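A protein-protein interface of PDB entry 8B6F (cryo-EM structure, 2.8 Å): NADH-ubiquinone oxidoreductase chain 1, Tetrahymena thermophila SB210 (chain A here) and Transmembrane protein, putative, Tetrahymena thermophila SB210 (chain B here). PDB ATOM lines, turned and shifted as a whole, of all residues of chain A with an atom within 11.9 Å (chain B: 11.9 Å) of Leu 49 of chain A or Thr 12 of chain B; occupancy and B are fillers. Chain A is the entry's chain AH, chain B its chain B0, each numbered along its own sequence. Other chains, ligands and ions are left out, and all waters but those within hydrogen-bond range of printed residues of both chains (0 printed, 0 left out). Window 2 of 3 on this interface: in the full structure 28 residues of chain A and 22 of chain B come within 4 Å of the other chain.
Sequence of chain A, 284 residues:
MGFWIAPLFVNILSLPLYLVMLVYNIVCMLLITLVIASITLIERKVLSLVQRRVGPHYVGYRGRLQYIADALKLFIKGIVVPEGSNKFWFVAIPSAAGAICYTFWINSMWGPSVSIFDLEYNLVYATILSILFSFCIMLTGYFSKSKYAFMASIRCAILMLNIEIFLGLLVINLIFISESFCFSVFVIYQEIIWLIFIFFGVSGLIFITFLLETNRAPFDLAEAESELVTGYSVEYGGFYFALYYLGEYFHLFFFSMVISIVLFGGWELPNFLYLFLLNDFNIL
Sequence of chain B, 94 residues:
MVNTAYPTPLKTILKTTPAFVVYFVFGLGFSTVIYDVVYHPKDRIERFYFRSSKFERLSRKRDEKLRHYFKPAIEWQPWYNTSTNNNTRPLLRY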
ATOM      1  N   THR A  40     -33.670 -31.425  31.566  1.00  0.00           N
ATOM      2  CA  THR A  40     -34.401 -30.367  30.876  1.00  0.00           C
ATOM      3  C   THR A  40     -33.668 -29.039  30.992  1.00  0.00           C
ATOM      4  O   THR A  40     -33.561 -28.293  30.013  1.00  0.00           O
ATOM      5  CB  THR A  40     -35.816 -30.239  31.440  1.00  0.00           C
ATOM      6  OG1 THR A  40     -35.753 -29.930  32.838  1.00  0.00           O
ATOM      7  CG2 THR A  40     -36.599 -31.524  31.237  1.00  0.00           C
ATOM      8  N   LEU A  41     -33.162 -28.719  32.184  1.00  0.00           N
ATOM      9  CA  LEU A  41     -32.395 -27.489  32.348  1.00  0.00           C
ATOM     10  C   LEU A  41     -31.148 -27.510  31.472  1.00  0.00           C
ATOM     11  O   LEU A  41     -30.796 -26.501  30.852  1.00  0.00           O
ATOM     12  CB  LEU A  41     -32.017 -27.289  33.815  1.00  0.00           C
ATOM     13  CG  LEU A  41     -31.206 -26.026  34.117  1.00  0.00           C
ATOM     14  CD1 LEU A  41     -31.960 -24.780  33.690  1.00  0.00           C
ATOM     15  CD2 LEU A  41     -30.850 -25.955  35.590  1.00  0.00           C
ATOM     16  N   ILE A  42     -30.469 -28.657  31.409  1.00  0.00           N
ATOM     17  CA  ILE A  42     -29.292 -28.785  30.555  1.00  0.00           C
ATOM     18  C   ILE A  42     -29.670 -28.559  29.099  1.00  0.00           C
ATOM     19  O   ILE A  42     -28.944 -27.897  28.349  1.00  0.00           O
ATOM     20  CB  ILE A  42     -28.632 -30.163  30.756  1.00  0.00           C
ATOM     21  CG1 ILE A  42     -27.930 -30.227  32.113  1.00  0.00           C
ATOM     22  CG2 ILE A  42     -27.662 -30.470  29.619  1.00  0.00           C
ATOM     23  CD1 ILE A  42     -27.425 -31.602  32.487  1.00  0.00           C
ATOM     24  N   GLU A  43     -30.813 -29.096  28.676  1.00  0.00           N
ATOM     25  CA  GLU A  43     -31.248 -28.910  27.298  1.00  0.00           C
ATOM     26  C   GLU A  43     -31.467 -27.436  26.991  1.00  0.00           C
ATOM     27  O   GLU A  43     -31.043 -26.940  25.942  1.00  0.00           O
ATOM     28  CB  GLU A  43     -32.515 -29.727  27.043  1.00  0.00           C
ATOM     29  CG  GLU A  43     -33.204 -29.436  25.721  1.00  0.00           C
ATOM     30  CD  GLU A  43     -34.202 -28.300  25.813  1.00  0.00           C
ATOM     31  OE1 GLU A  43     -34.313 -27.684  26.893  1.00  0.00           O
ATOM     32  OE2 GLU A  43     -34.883 -28.026  24.802  1.00  0.00           O
ATOM     33  N   ARG A  44     -32.138 -26.718  27.889  1.00  0.00           N
ATOM     34  CA  ARG A  44     -32.345 -25.293  27.664  1.00  0.00           C
ATOM     35  C   ARG A  44     -31.016 -24.550  27.590  1.00  0.00           C
ATOM     36  O   ARG A  44     -30.826 -23.690  26.722  1.00  0.00           O
ATOM     37  CB  ARG A  44     -33.232 -24.719  28.768  1.00  0.00           C
ATOM     38  CG  ARG A  44     -34.709 -24.768  28.421  1.00  0.00           C
ATOM     39  CD  ARG A  44     -35.579 -24.199  29.520  1.00  0.00           C
ATOM     40  NE  ARG A  44     -35.523 -25.011  30.730  1.00  0.00           N
ATOM     41  CZ  ARG A  44     -36.374 -24.906  31.741  1.00  0.00           C
ATOM     42  NH1 ARG A  44     -37.373 -24.039  31.716  1.00  0.00           N
ATOM     43  NH2 ARG A  44     -36.223 -25.694  32.801  1.00  0.00           N
ATOM     44  N   LYS A  45     -30.084 -24.865  28.494  1.00  0.00           N
ATOM     45  CA  LYS A  45     -28.799 -24.169  28.504  1.00  0.00           C
ATOM     46  C   LYS A  45     -27.970 -24.487  27.264  1.00  0.00           C
ATOM     47  O   LYS A  45     -27.306 -23.601  26.716  1.00  0.00           O
ATOM     48  CB  LYS A  45     -28.019 -24.528  29.768  1.00  0.00           C
ATOM     49  CG  LYS A  45     -28.511 -23.828  31.025  1.00  0.00           C
ATOM     50  CD  LYS A  45     -28.214 -22.339  30.990  1.00  0.00           C
ATOM     51  CE  LYS A  45     -28.607 -21.668  32.293  1.00  0.00           C
ATOM     52  NZ  LYS A  45     -28.269 -20.219  32.292  1.00  0.00           N
ATOM     53  N   VAL A  46     -27.991 -25.740  26.807  1.00  0.00           N
ATOM     54  CA  VAL A  46     -27.221 -26.103  25.620  1.00  0.00           C
ATOM     55  C   VAL A  46     -27.793 -25.424  24.383  1.00  0.00           C
ATOM     56  O   VAL A  46     -27.049 -24.915  23.538  1.00  0.00           O
ATOM     57  CB  VAL A  46     -27.172 -27.633  25.458  1.00  0.00           C
ATOM     58  CG1 VAL A  46     -26.606 -28.022  24.096  1.00  0.00           C
ATOM     59  CG2 VAL A  46     -26.334 -28.250  26.561  1.00  0.00           C
ATOM     60  N   LEU A  47     -29.119 -25.398  24.256  1.00  0.00           N
ATOM     61  CA  LEU A  47     -29.731 -24.671  23.151  1.00  0.00           C
ATOM     62  C   LEU A  47     -29.419 -23.184  23.243  1.00  0.00           C
ATOM     63  O   LEU A  47     -29.225 -22.517  22.221  1.00  0.00           O
ATOM     64  CB  LEU A  47     -31.241 -24.908  23.131  1.00  0.00           C
ATOM     65  CG  LEU A  47     -31.704 -26.322  22.765  1.00  0.00           C
ATOM     66  CD1 LEU A  47     -33.219 -26.410  22.802  1.00  0.00           C
ATOM     67  CD2 LEU A  47     -31.186 -26.745  21.401  1.00  0.00           C
ATOM     68  N   SER A  48     -29.359 -22.647  24.462  1.00  0.00           N
ATOM     69  CA  SER A  48     -28.988 -21.247  24.627  1.00  0.00           C
ATOM     70  C   SER A  48     -27.568 -20.995  24.141  1.00  0.00           C
ATOM     71  O   SER A  48     -27.296 -19.973  23.504  1.00  0.00           O
ATOM     72  CB  SER A  48     -29.133 -20.846  26.094  1.00  0.00           C
ATOM     73  OG  SER A  48     -30.455 -21.083  26.547  1.00  0.00           O
ATOM     74  N   LEU A  49     -26.646 -21.913  24.435  1.00  0.00           N
ATOM     75  CA  LEU A  49     -25.287 -21.774  23.922  1.00  0.00           C
ATOM     76  C   LEU A  49     -25.265 -21.836  22.401  1.00  0.00           C
ATOM     77  O   LEU A  49     -24.567 -21.052  21.750  1.00  0.00           O
ATOM     78  CB  LEU A  49     -24.386 -22.863  24.501  1.00  0.00           C
ATOM     79  CG  LEU A  49     -23.976 -22.734  25.967  1.00  0.00           C
ATOM     80  CD1 LEU A  49     -23.091 -23.901  26.350  1.00  0.00           C
ATOM     81  CD2 LEU A  49     -23.269 -21.418  26.245  1.00  0.00           C
ATOM     82  N   VAL A  50     -26.023 -22.764  21.818  1.00  0.00           N
ATOM     83  CA  VAL A  50     -26.029 -22.903  20.366  1.00  0.00           C
ATOM     84  C   VAL A  50     -26.603 -21.649  19.721  1.00  0.00           C
ATOM     85  O   VAL A  50     -26.163 -21.227  18.646  1.00  0.00           O
ATOM     86  CB  VAL A  50     -26.813 -24.162  19.953  1.00  0.00           C
ATOM     87  CG1 VAL A  50     -27.024 -24.199  18.448  1.00  0.00           C
ATOM     88  CG2 VAL A  50     -26.093 -25.414  20.418  1.00  0.00           C
ATOM     89  N   GLN A  51     -27.594 -21.038  20.363  1.00  0.00           N
ATOM     90  CA  GLN A  51     -28.258 -19.859  19.827  1.00  0.00           C
ATOM     91  C   GLN A  51     -27.664 -18.556  20.342  1.00  0.00           C
ATOM     92  O   GLN A  51     -28.193 -17.485  20.032  1.00  0.00           O
ATOM     93  CB  GLN A  51     -29.751 -19.922  20.161  1.00  0.00           C
ATOM     94  CG  GLN A  51     -30.432 -21.170  19.614  1.00  0.00           C
ATOM     95  CD  GLN A  51     -31.794 -21.409  20.221  1.00  0.00           C
ATOM     96  OE1 GLN A  51     -32.183 -20.753  21.183  1.00  0.00           O
ATOM     97  NE2 GLN A  51     -32.529 -22.359  19.657  1.00  0.00           N
ATOM     98  N   ARG A  52     -26.586 -18.623  21.122  1.00  0.00           N
ATOM     99  CA  ARG A  52     -25.886 -17.441  21.622  1.00  0.00           C
ATOM    100  C   ARG A  52     -26.817 -16.556  22.454  1.00  0.00           C
ATOM    101  O   ARG A  52     -27.070 -15.394  22.135  1.00  0.00           O
ATOM    102  CB  ARG A  52     -25.266 -16.661  20.462  1.00  0.00           C
ATOM    103  CG  ARG A  52     -24.323 -17.496  19.610  1.00  0.00           C
ATOM    104  CD  ARG A  52     -23.824 -16.689  18.438  1.00  0.00           C
ATOM    105  NE  ARG A  52     -24.085 -17.334  17.158  1.00  0.00           N
ATOM    106  CZ  ARG A  52     -23.261 -18.180  16.555  1.00  0.00           C
ATOM    107  NH1 ARG A  52     -22.108 -18.531  17.100  1.00  0.00           N
ATOM    108  NH2 ARG A  52     -23.600 -18.682  15.372  1.00  0.00           N
ATOM    109  N   ARG A  53     -27.322 -17.134  23.541  1.00  0.00           N
ATOM    110  CA  ARG A  53     -28.148 -16.408  24.491  1.00  0.00           C
ATOM    111  C   ARG A  53     -27.865 -16.942  25.886  1.00  0.00           C
ATOM    112  O   ARG A  53     -27.335 -18.044  26.052  1.00  0.00           O
ATOM    113  CB  ARG A  53     -29.640 -16.521  24.154  1.00  0.00           C
ATOM    114  CG  ARG A  53     -30.140 -17.944  23.999  1.00  0.00           C
ATOM    115  CD  ARG A  53     -31.563 -17.965  23.469  1.00  0.00           C
ATOM    116  NE  ARG A  53     -32.073 -19.322  23.320  1.00  0.00           N
ATOM    117  CZ  ARG A  53     -32.698 -20.003  24.271  1.00  0.00           C
ATOM    118  NH1 ARG A  53     -32.909 -19.484  25.469  1.00  0.00           N
ATOM    119  NH2 ARG A  53     -33.123 -21.236  24.015  1.00  0.00           N
ATOM    120  N   VAL A  54     -28.216 -16.143  26.891  1.00  0.00           N
ATOM    121  CA  VAL A  54     -27.916 -16.509  28.272  1.00  0.00           C
ATOM    122  C   VAL A  54     -28.741 -17.718  28.696  1.00  0.00           C
ATOM    123  O   VAL A  54     -28.218 -18.668  29.289  1.00  0.00           O
ATOM    124  CB  VAL A  54     -28.152 -15.310  29.207  1.00  0.00           C
ATOM    125  CG1 VAL A  54     -27.937 -15.706  30.659  1.00  0.00           C
ATOM    126  CG2 VAL A  54     -27.241 -14.159  28.828  1.00  0.00           C
ATOM    127  N   GLY A  55     -30.036 -17.705  28.398  1.00  0.00           N
ATOM    128  CA  GLY A  55     -30.927 -18.743  28.856  1.00  0.00           C
ATOM    129  C   GLY A  55     -31.422 -18.462  30.259  1.00  0.00           C
ATOM    130  O   GLY A  55     -31.210 -17.377  30.804  1.00  0.00           O
ATOM    131  N   PRO A  56     -32.091 -19.442  30.876  1.00  0.00           N
ATOM    132  CA  PRO A  56     -32.629 -19.231  32.229  1.00  0.00           C
ATOM    133  C   PRO A  56     -31.594 -18.671  33.191  1.00  0.00           C
ATOM    134  O   PRO A  56     -30.583 -19.315  33.476  1.00  0.00           O
ATOM    135  CB  PRO A  56     -33.081 -20.636  32.645  1.00  0.00           C
ATOM    136  CG  PRO A  56     -33.384 -21.324  31.363  1.00  0.00           C
ATOM    137  CD  PRO A  56     -32.400 -20.787  30.361  1.00  0.00           C
ATOM    138  N   HIS A  57     -31.847 -17.462  33.695  1.00  0.00           N
ATOM    139  CA  HIS A  57     -30.872 -16.766  34.523  1.00  0.00           C
ATOM    140  C   HIS A  57     -31.457 -16.078  35.748  1.00  0.00           C
ATOM    141  O   HIS A  57     -30.681 -15.690  36.626  1.00  0.00           O
ATOM    142  CB  HIS A  57     -30.130 -15.721  33.676  1.00  0.00           C
ATOM    143  CG  HIS A  57     -28.861 -15.228  34.296  1.00  0.00           C
ATOM    144  ND1 HIS A  57     -28.778 -14.027  34.967  1.00  0.00           N
ATOM    145  CD2 HIS A  57     -27.621 -15.768  34.337  1.00  0.00           C
ATOM    146  CE1 HIS A  57     -27.543 -13.852  35.400  1.00  0.00           C
ATOM    147  NE2 HIS A  57     -26.821 -14.894  35.032  1.00  0.00           N
ATOM    148  N   ALA B   5      -7.900 -13.174  32.100  1.00  0.00           N
ATOM    149  CA  ALA B   5      -9.269 -13.645  31.991  1.00  0.00           C
ATOM    150  C   ALA B   5      -9.323 -14.961  31.218  1.00  0.00           C
ATOM    151  O   ALA B   5      -8.367 -15.366  30.551  1.00  0.00           O
ATOM    152  CB  ALA B   5     -10.141 -12.592  31.310  1.00  0.00           C
ATOM    153  N   TYR B   6     -10.464 -15.636  31.319  1.00  0.00           N
ATOM    154  CA  TYR B   6     -10.657 -16.881  30.598  1.00  0.00           C
ATOM    155  C   TYR B   6     -10.702 -16.619  29.093  1.00  0.00           C
ATOM    156  O   TYR B   6     -11.056 -15.522  28.656  1.00  0.00           O
ATOM    157  CB  TYR B   6     -11.955 -17.559  31.026  1.00  0.00           C
ATOM    158  CG  TYR B   6     -11.924 -18.182  32.401  1.00  0.00           C
ATOM    159  CD1 TYR B   6     -11.890 -17.396  33.543  1.00  0.00           C
ATOM    160  CD2 TYR B   6     -11.971 -19.559  32.556  1.00  0.00           C
ATOM    161  CE1 TYR B   6     -11.878 -17.965  34.802  1.00  0.00           C
ATOM    162  CE2 TYR B   6     -11.960 -20.138  33.807  1.00  0.00           C
ATOM    163  CZ  TYR B   6     -11.914 -19.336  34.926  1.00  0.00           C
ATOM    164  OH  TYR B   6     -11.904 -19.909  36.175  1.00  0.00           O
ATOM    165  N   PRO B   7     -10.340 -17.608  28.278  1.00  0.00           N
ATOM    166  CA  PRO B   7     -10.608 -17.499  26.842  1.00  0.00           C
ATOM    167  C   PRO B   7     -12.100 -17.375  26.577  1.00  0.00           C
ATOM    168  O   PRO B   7     -12.932 -17.915  27.308  1.00  0.00           O
ATOM    169  CB  PRO B   7     -10.043 -18.806  26.272  1.00  0.00           C
ATOM    170  CG  PRO B   7      -9.032 -19.244  27.260  1.00  0.00           C
ATOM    171  CD  PRO B   7      -9.542 -18.803  28.598  1.00  0.00           C
ATOM    172  N   THR B   8     -12.432 -16.645  25.517  1.00  0.00           N
ATOM    173  CA  THR B   8     -13.836 -16.433  25.173  1.00  0.00           C
ATOM    174  C   THR B   8     -14.597 -17.736  24.973  1.00  0.00           C
ATOM    175  O   THR B   8     -15.694 -17.876  25.540  1.00  0.00           O
ATOM    176  CB  THR B   8     -13.926 -15.544  23.930  1.00  0.00           C
ATOM    177  OG1 THR B   8     -13.685 -14.180  24.297  1.00  0.00           O
ATOM    178  CG2 THR B   8     -15.293 -15.663  23.270  1.00  0.00           C
ATOM    179  N   PRO B   9     -14.111 -18.706  24.194  1.00  0.00           N
ATOM    180  CA  PRO B   9     -14.886 -19.948  24.038  1.00  0.00           C
ATOM    181  C   PRO B   9     -15.125 -20.670  25.349  1.00  0.00           C
ATOM    182  O   PRO B   9     -16.241 -21.142  25.595  1.00  0.00           O
ATOM    183  CB  PRO B   9     -14.027 -20.780  23.072  1.00  0.00           C
ATOM    184  CG  PRO B   9     -12.673 -20.184  23.138  1.00  0.00           C
ATOM    185  CD  PRO B   9     -12.879 -18.728  23.389  1.00  0.00           C
ATOM    186  N   LEU B  10     -14.109 -20.767  26.203  1.00  0.00           N
ATOM    187  CA  LEU B  10     -14.284 -21.447  27.481  1.00  0.00           C
ATOM    188  C   LEU B  10     -15.270 -20.702  28.373  1.00  0.00           C
ATOM    189  O   LEU B  10     -16.117 -21.323  29.023  1.00  0.00           O
ATOM    190  CB  LEU B  10     -12.936 -21.604  28.183  1.00  0.00           C
ATOM    191  CG  LEU B  10     -12.945 -22.445  29.462  1.00  0.00           C
ATOM    192  CD1 LEU B  10     -13.389 -23.871  29.177  1.00  0.00           C
ATOM    193  CD2 LEU B  10     -11.573 -22.437  30.107  1.00  0.00           C
ATOM    194  N   LYS B  11     -15.190 -19.371  28.404  1.00  0.00           N
ATOM    195  CA  LYS B  11     -16.116 -18.595  29.222  1.00  0.00           C
ATOM    196  C   LYS B  11     -17.554 -18.779  28.752  1.00  0.00           C
ATOM    197  O   LYS B  11     -18.474 -18.882  29.571  1.00  0.00           O
ATOM    198  CB  LYS B  11     -15.732 -17.116  29.195  1.00  0.00           C
ATOM    199  CG  LYS B  11     -16.217 -16.347  30.410  1.00  0.00           C
ATOM    200  CD  LYS B  11     -16.065 -14.849  30.238  1.00  0.00           C
ATOM    201  CE  LYS B  11     -17.142 -14.289  29.324  1.00  0.00           C
ATOM    202  NZ  LYS B  11     -17.098 -12.801  29.267  1.00  0.00           N
ATOM    203  N   THR B  12     -17.768 -18.814  27.439  1.00  0.00           N
ATOM    204  CA  THR B  12     -19.105 -19.066  26.914  1.00  0.00           C
ATOM    205  C   THR B  12     -19.590 -20.462  27.293  1.00  0.00           C
ATOM    206  O   THR B  12     -20.750 -20.640  27.676  1.00  0.00           O
ATOM    207  CB  THR B  12     -19.108 -18.891  25.394  1.00  0.00           C
ATOM    208  OG1 THR B  12     -18.726 -17.551  25.063  1.00  0.00           O
ATOM    209  CG2 THR B  12     -20.485 -19.174  24.812  1.00  0.00           C
ATOM    210  N   ILE B  13     -18.714 -21.463  27.193  1.00  0.00           N
ATOM    211  CA  ILE B  13     -19.111 -22.835  27.492  1.00  0.00           C
ATOM    212  C   ILE B  13     -19.471 -22.986  28.963  1.00  0.00           C
ATOM    213  O   ILE B  13     -20.377 -23.748  29.318  1.00  0.00           O
ATOM    214  CB  ILE B  13     -17.979 -23.805  27.108  1.00  0.00           C
ATOM    215  CG1 ILE B  13     -17.810 -23.866  25.596  1.00  0.00           C
ATOM    216  CG2 ILE B  13     -18.260 -25.206  27.652  1.00  0.00           C
ATOM    217  CD1 ILE B  13     -16.567 -24.607  25.188  1.00  0.00           C
ATOM    218  N   LEU B  14     -18.772 -22.271  29.843  1.00  0.00           N
ATOM    219  CA  LEU B  14     -18.946 -22.476  31.275  1.00  0.00           C
ATOM    220  C   LEU B  14     -20.334 -22.096  31.767  1.00  0.00           C
ATOM    221  O   LEU B  14     -20.687 -22.450  32.896  1.00  0.00           O
ATOM    222  CB  LEU B  14     -17.891 -21.679  32.043  1.00  0.00           C
ATOM    223  CG  LEU B  14     -16.462 -22.224  31.978  1.00  0.00           C
ATOM    224  CD1 LEU B  14     -15.482 -21.200  32.520  1.00  0.00           C
ATOM    225  CD2 LEU B  14     -16.332 -23.532  32.733  1.00  0.00           C
ATOM    226  N   LYS B  15     -21.128 -21.395  30.957  1.00  0.00           N
ATOM    227  CA  LYS B  15     -22.443 -20.957  31.414  1.00  0.00           C
ATOM    228  C   LYS B  15     -23.330 -22.142  31.774  1.00  0.00           C
ATOM    229  O   LYS B  15     -24.059 -22.099  32.770  1.00  0.00           O
ATOM    230  CB  LYS B  15     -23.107 -20.099  30.340  1.00  0.00           C
ATOM    231  CG  LYS B  15     -22.433 -18.758  30.125  1.00  0.00           C
ATOM    232  CD  LYS B  15     -22.758 -18.188  28.758  1.00  0.00           C
ATOM    233  CE  LYS B  15     -24.251 -18.011  28.562  1.00  0.00           C
ATOM    234  NZ  LYS B  15     -24.543 -17.423  27.230  1.00  0.00           N
ATOM    235  N   THR B  16     -23.289 -23.204  30.973  1.00  0.00           N
ATOM    236  CA  THR B  16     -24.145 -24.364  31.180  1.00  0.00           C
ATOM    237  C   THR B  16     -23.555 -25.376  32.152  1.00  0.00           C
ATOM    238  O   THR B  16     -24.187 -26.407  32.408  1.00  0.00           O
ATOM    239  CB  THR B  16     -24.426 -25.057  29.842  1.00  0.00           C
ATOM    240  OG1 THR B  16     -25.378 -26.109  30.038  1.00  0.00           O
ATOM    241  CG2 THR B  16     -23.149 -25.646  29.254  1.00  0.00           C
ATOM    242  N   THR B  17     -22.365 -25.120  32.685  1.00  0.00           N
ATOM    243  CA  THR B  17     -21.732 -26.091  33.571  1.00  0.00           C
ATOM    244  C   THR B  17     -22.526 -26.362  34.843  1.00  0.00           C
ATOM    245  O   THR B  17     -22.624 -27.538  35.234  1.00  0.00           O
ATOM    246  CB  THR B  17     -20.312 -25.632  33.914  1.00  0.00           C
ATOM    247  OG1 THR B  17     -19.517 -25.595  32.723  1.00  0.00           O
ATOM    248  CG2 THR B  17     -19.685 -26.587  34.905  1.00  0.00           C
ATOM    249  N   PRO B  18     -23.089 -25.367  35.532  1.00  0.00           N
ATOM    250  CA  PRO B  18     -23.845 -25.683  36.756  1.00  0.00           C
ATOM    251  C   PRO B  18     -24.953 -26.693  36.529  1.00  0.00           C
ATOM    252  O   PRO B  18     -25.228 -27.513  37.412  1.00  0.00           O
ATOM    253  CB  PRO B  18     -24.395 -24.316  37.187  1.00  0.00           C
ATOM    254  CG  PRO B  18     -23.464 -23.328  36.587  1.00  0.00           C
ATOM    255  CD  PRO B  18     -23.020 -23.917  35.286  1.00  0.00           C
ATOM    256  N   ALA B  19     -25.601 -26.657  35.365  1.00  0.00           N
ATOM    257  CA  ALA B  19     -26.590 -27.678  35.047  1.00  0.00           C
ATOM    258  C   ALA B  19     -25.951 -29.061  35.001  1.00  0.00           C
ATOM    259  O   ALA B  19     -26.530 -30.038  35.488  1.00  0.00           O
ATOM    260  CB  ALA B  19     -27.268 -27.347  33.719  1.00  0.00           C
ATOM    261  N   PHE B  20     -24.754 -29.165  34.416  1.00  0.00           N
ATOM    262  CA  PHE B  20     -24.040 -30.439  34.412  1.00  0.00           C
ATOM    263  C   PHE B  20     -23.731 -30.901  35.830  1.00  0.00           C
ATOM    264  O   PHE B  20     -23.851 -32.089  36.143  1.00  0.00           O
ATOM    265  CB  PHE B  20     -22.740 -30.322  33.613  1.00  0.00           C
ATOM    266  CG  PHE B  20     -22.934 -30.014  32.154  1.00  0.00           C
ATOM    267  CD1 PHE B  20     -24.135 -30.274  31.519  1.00  0.00           C
ATOM    268  CD2 PHE B  20     -21.897 -29.475  31.414  1.00  0.00           C
ATOM    269  CE1 PHE B  20     -24.296 -29.995  30.178  1.00  0.00           C
ATOM    270  CE2 PHE B  20     -22.057 -29.195  30.073  1.00  0.00           C
ATOM    271  CZ  PHE B  20     -23.259 -29.453  29.455  1.00  0.00           C
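The backbone carbonyl oxygen (O) of Arg 53 of chain A sits at hydrogen-bond distance from the side-chain amino group (NZ) of Lys 15 of chain B (3.1 Å).
The backbone carbonyl oxygen of Val 54 of chain A sits at hydrogen-bond distance from the side-chain amino group of Lys 45 of chain A, at 3.4 Å. The backbone carbonyl oxygen of Pro 56 of chain A is in hydrogen-bond range of the side-chain amino group of Lys 45 of chain A, 2.8 Å away. The backbone NH (N) of Arg 53 of chain A is in hydrogen-bond range of the backbone carbonyl oxygen (O) of Ser 48 of chain A, at 2.8 Å. OE1 of Gln 51 of chain A lies within hydrogen-bond range of NE of Arg 53 of chain A, 2.6 Å away. The backbone carbonyl oxygen of Thr 8 of chain B is in hydrogen-bond range of the side-chain hydroxyl of Thr 12 of chain B (3.1 Å).
Among the printed residues, pairs that only touch across the chains: Ile 42 of chain A with Ala 19 of chain B, Ile 42 of chain A with Phe 20 of chain B, Lys 45 of chain A with Thr 16 of chain B, Leu 49 of chain A with Thr 12 of chain B, Leu 49 of chain A with Thr 16 of chain B and Val 54 of chain A with Lys 15 of chain B.
Of chain A, only Leu 49 comes within 4 Å of Thr 12 of chain B. No residue of chain B comes within 4 Å of Val 50 of chain A. No residue of chain B comes within 4 Å of Arg 52 of chain A. Arg 53 of chain A touches just one residue of chain B: Lys 15 (3.1 Å). No residue of chain A comes within 4 Å of Leu 10 of chain B. No residue of chain A comes within 4 Å of Lys 11 of chain B. Ile 13 of chain B touches none of the printed residues of chain A. No residue of chain A comes within 4 Å of Leu 14 of chain B. Of the printed residues of chain A, Lys 15 of chain B touches Arg 53 (3.1 Å) and Val 54 (3.6 Å). Of chain A, only Lys 45 (3.1 Å) and Leu 49 (3.4 Å) come within 4 Å of Thr 16 of chain B. Printed residues of chain A within 4 Å of Phe 20 of chain B: Ile 42 (3.4 Å). Of the printed residues of chain A, Ala 19 of chain B touches Ile 42 (3.4 Å). Of the printed residues of chain B, Val 54 of chain A touches Lys 15 (3.6 Å). The nearest residue of chain B that does not touch Leu 49 of chain A is Ile 13 of chain B (4.02 Å). The nearest printed residue of chain B that does not touch Val 54 of chain A is Thr 16 of chain B (6.9 Å).
Of the 18 printed residues of chain A, 5 touch a printed residue of chain B. Along chain A the printed residues that touch a printed residue of chain B span positions 42 to 54. Printed residues of chain B that touch a printed residue of chain A: Thr 12, Lys 15, Thr 16, Ala 19 and Phe 20. Hydrophobic or aromatic side chains of chain B that line the printed part of chain A: Ala 19 and Phe 20. Among the printed residues, no Asp or Glu carboxylate lies within 4 Å of a Lys or Arg side-chain nitrogen of the other chain.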
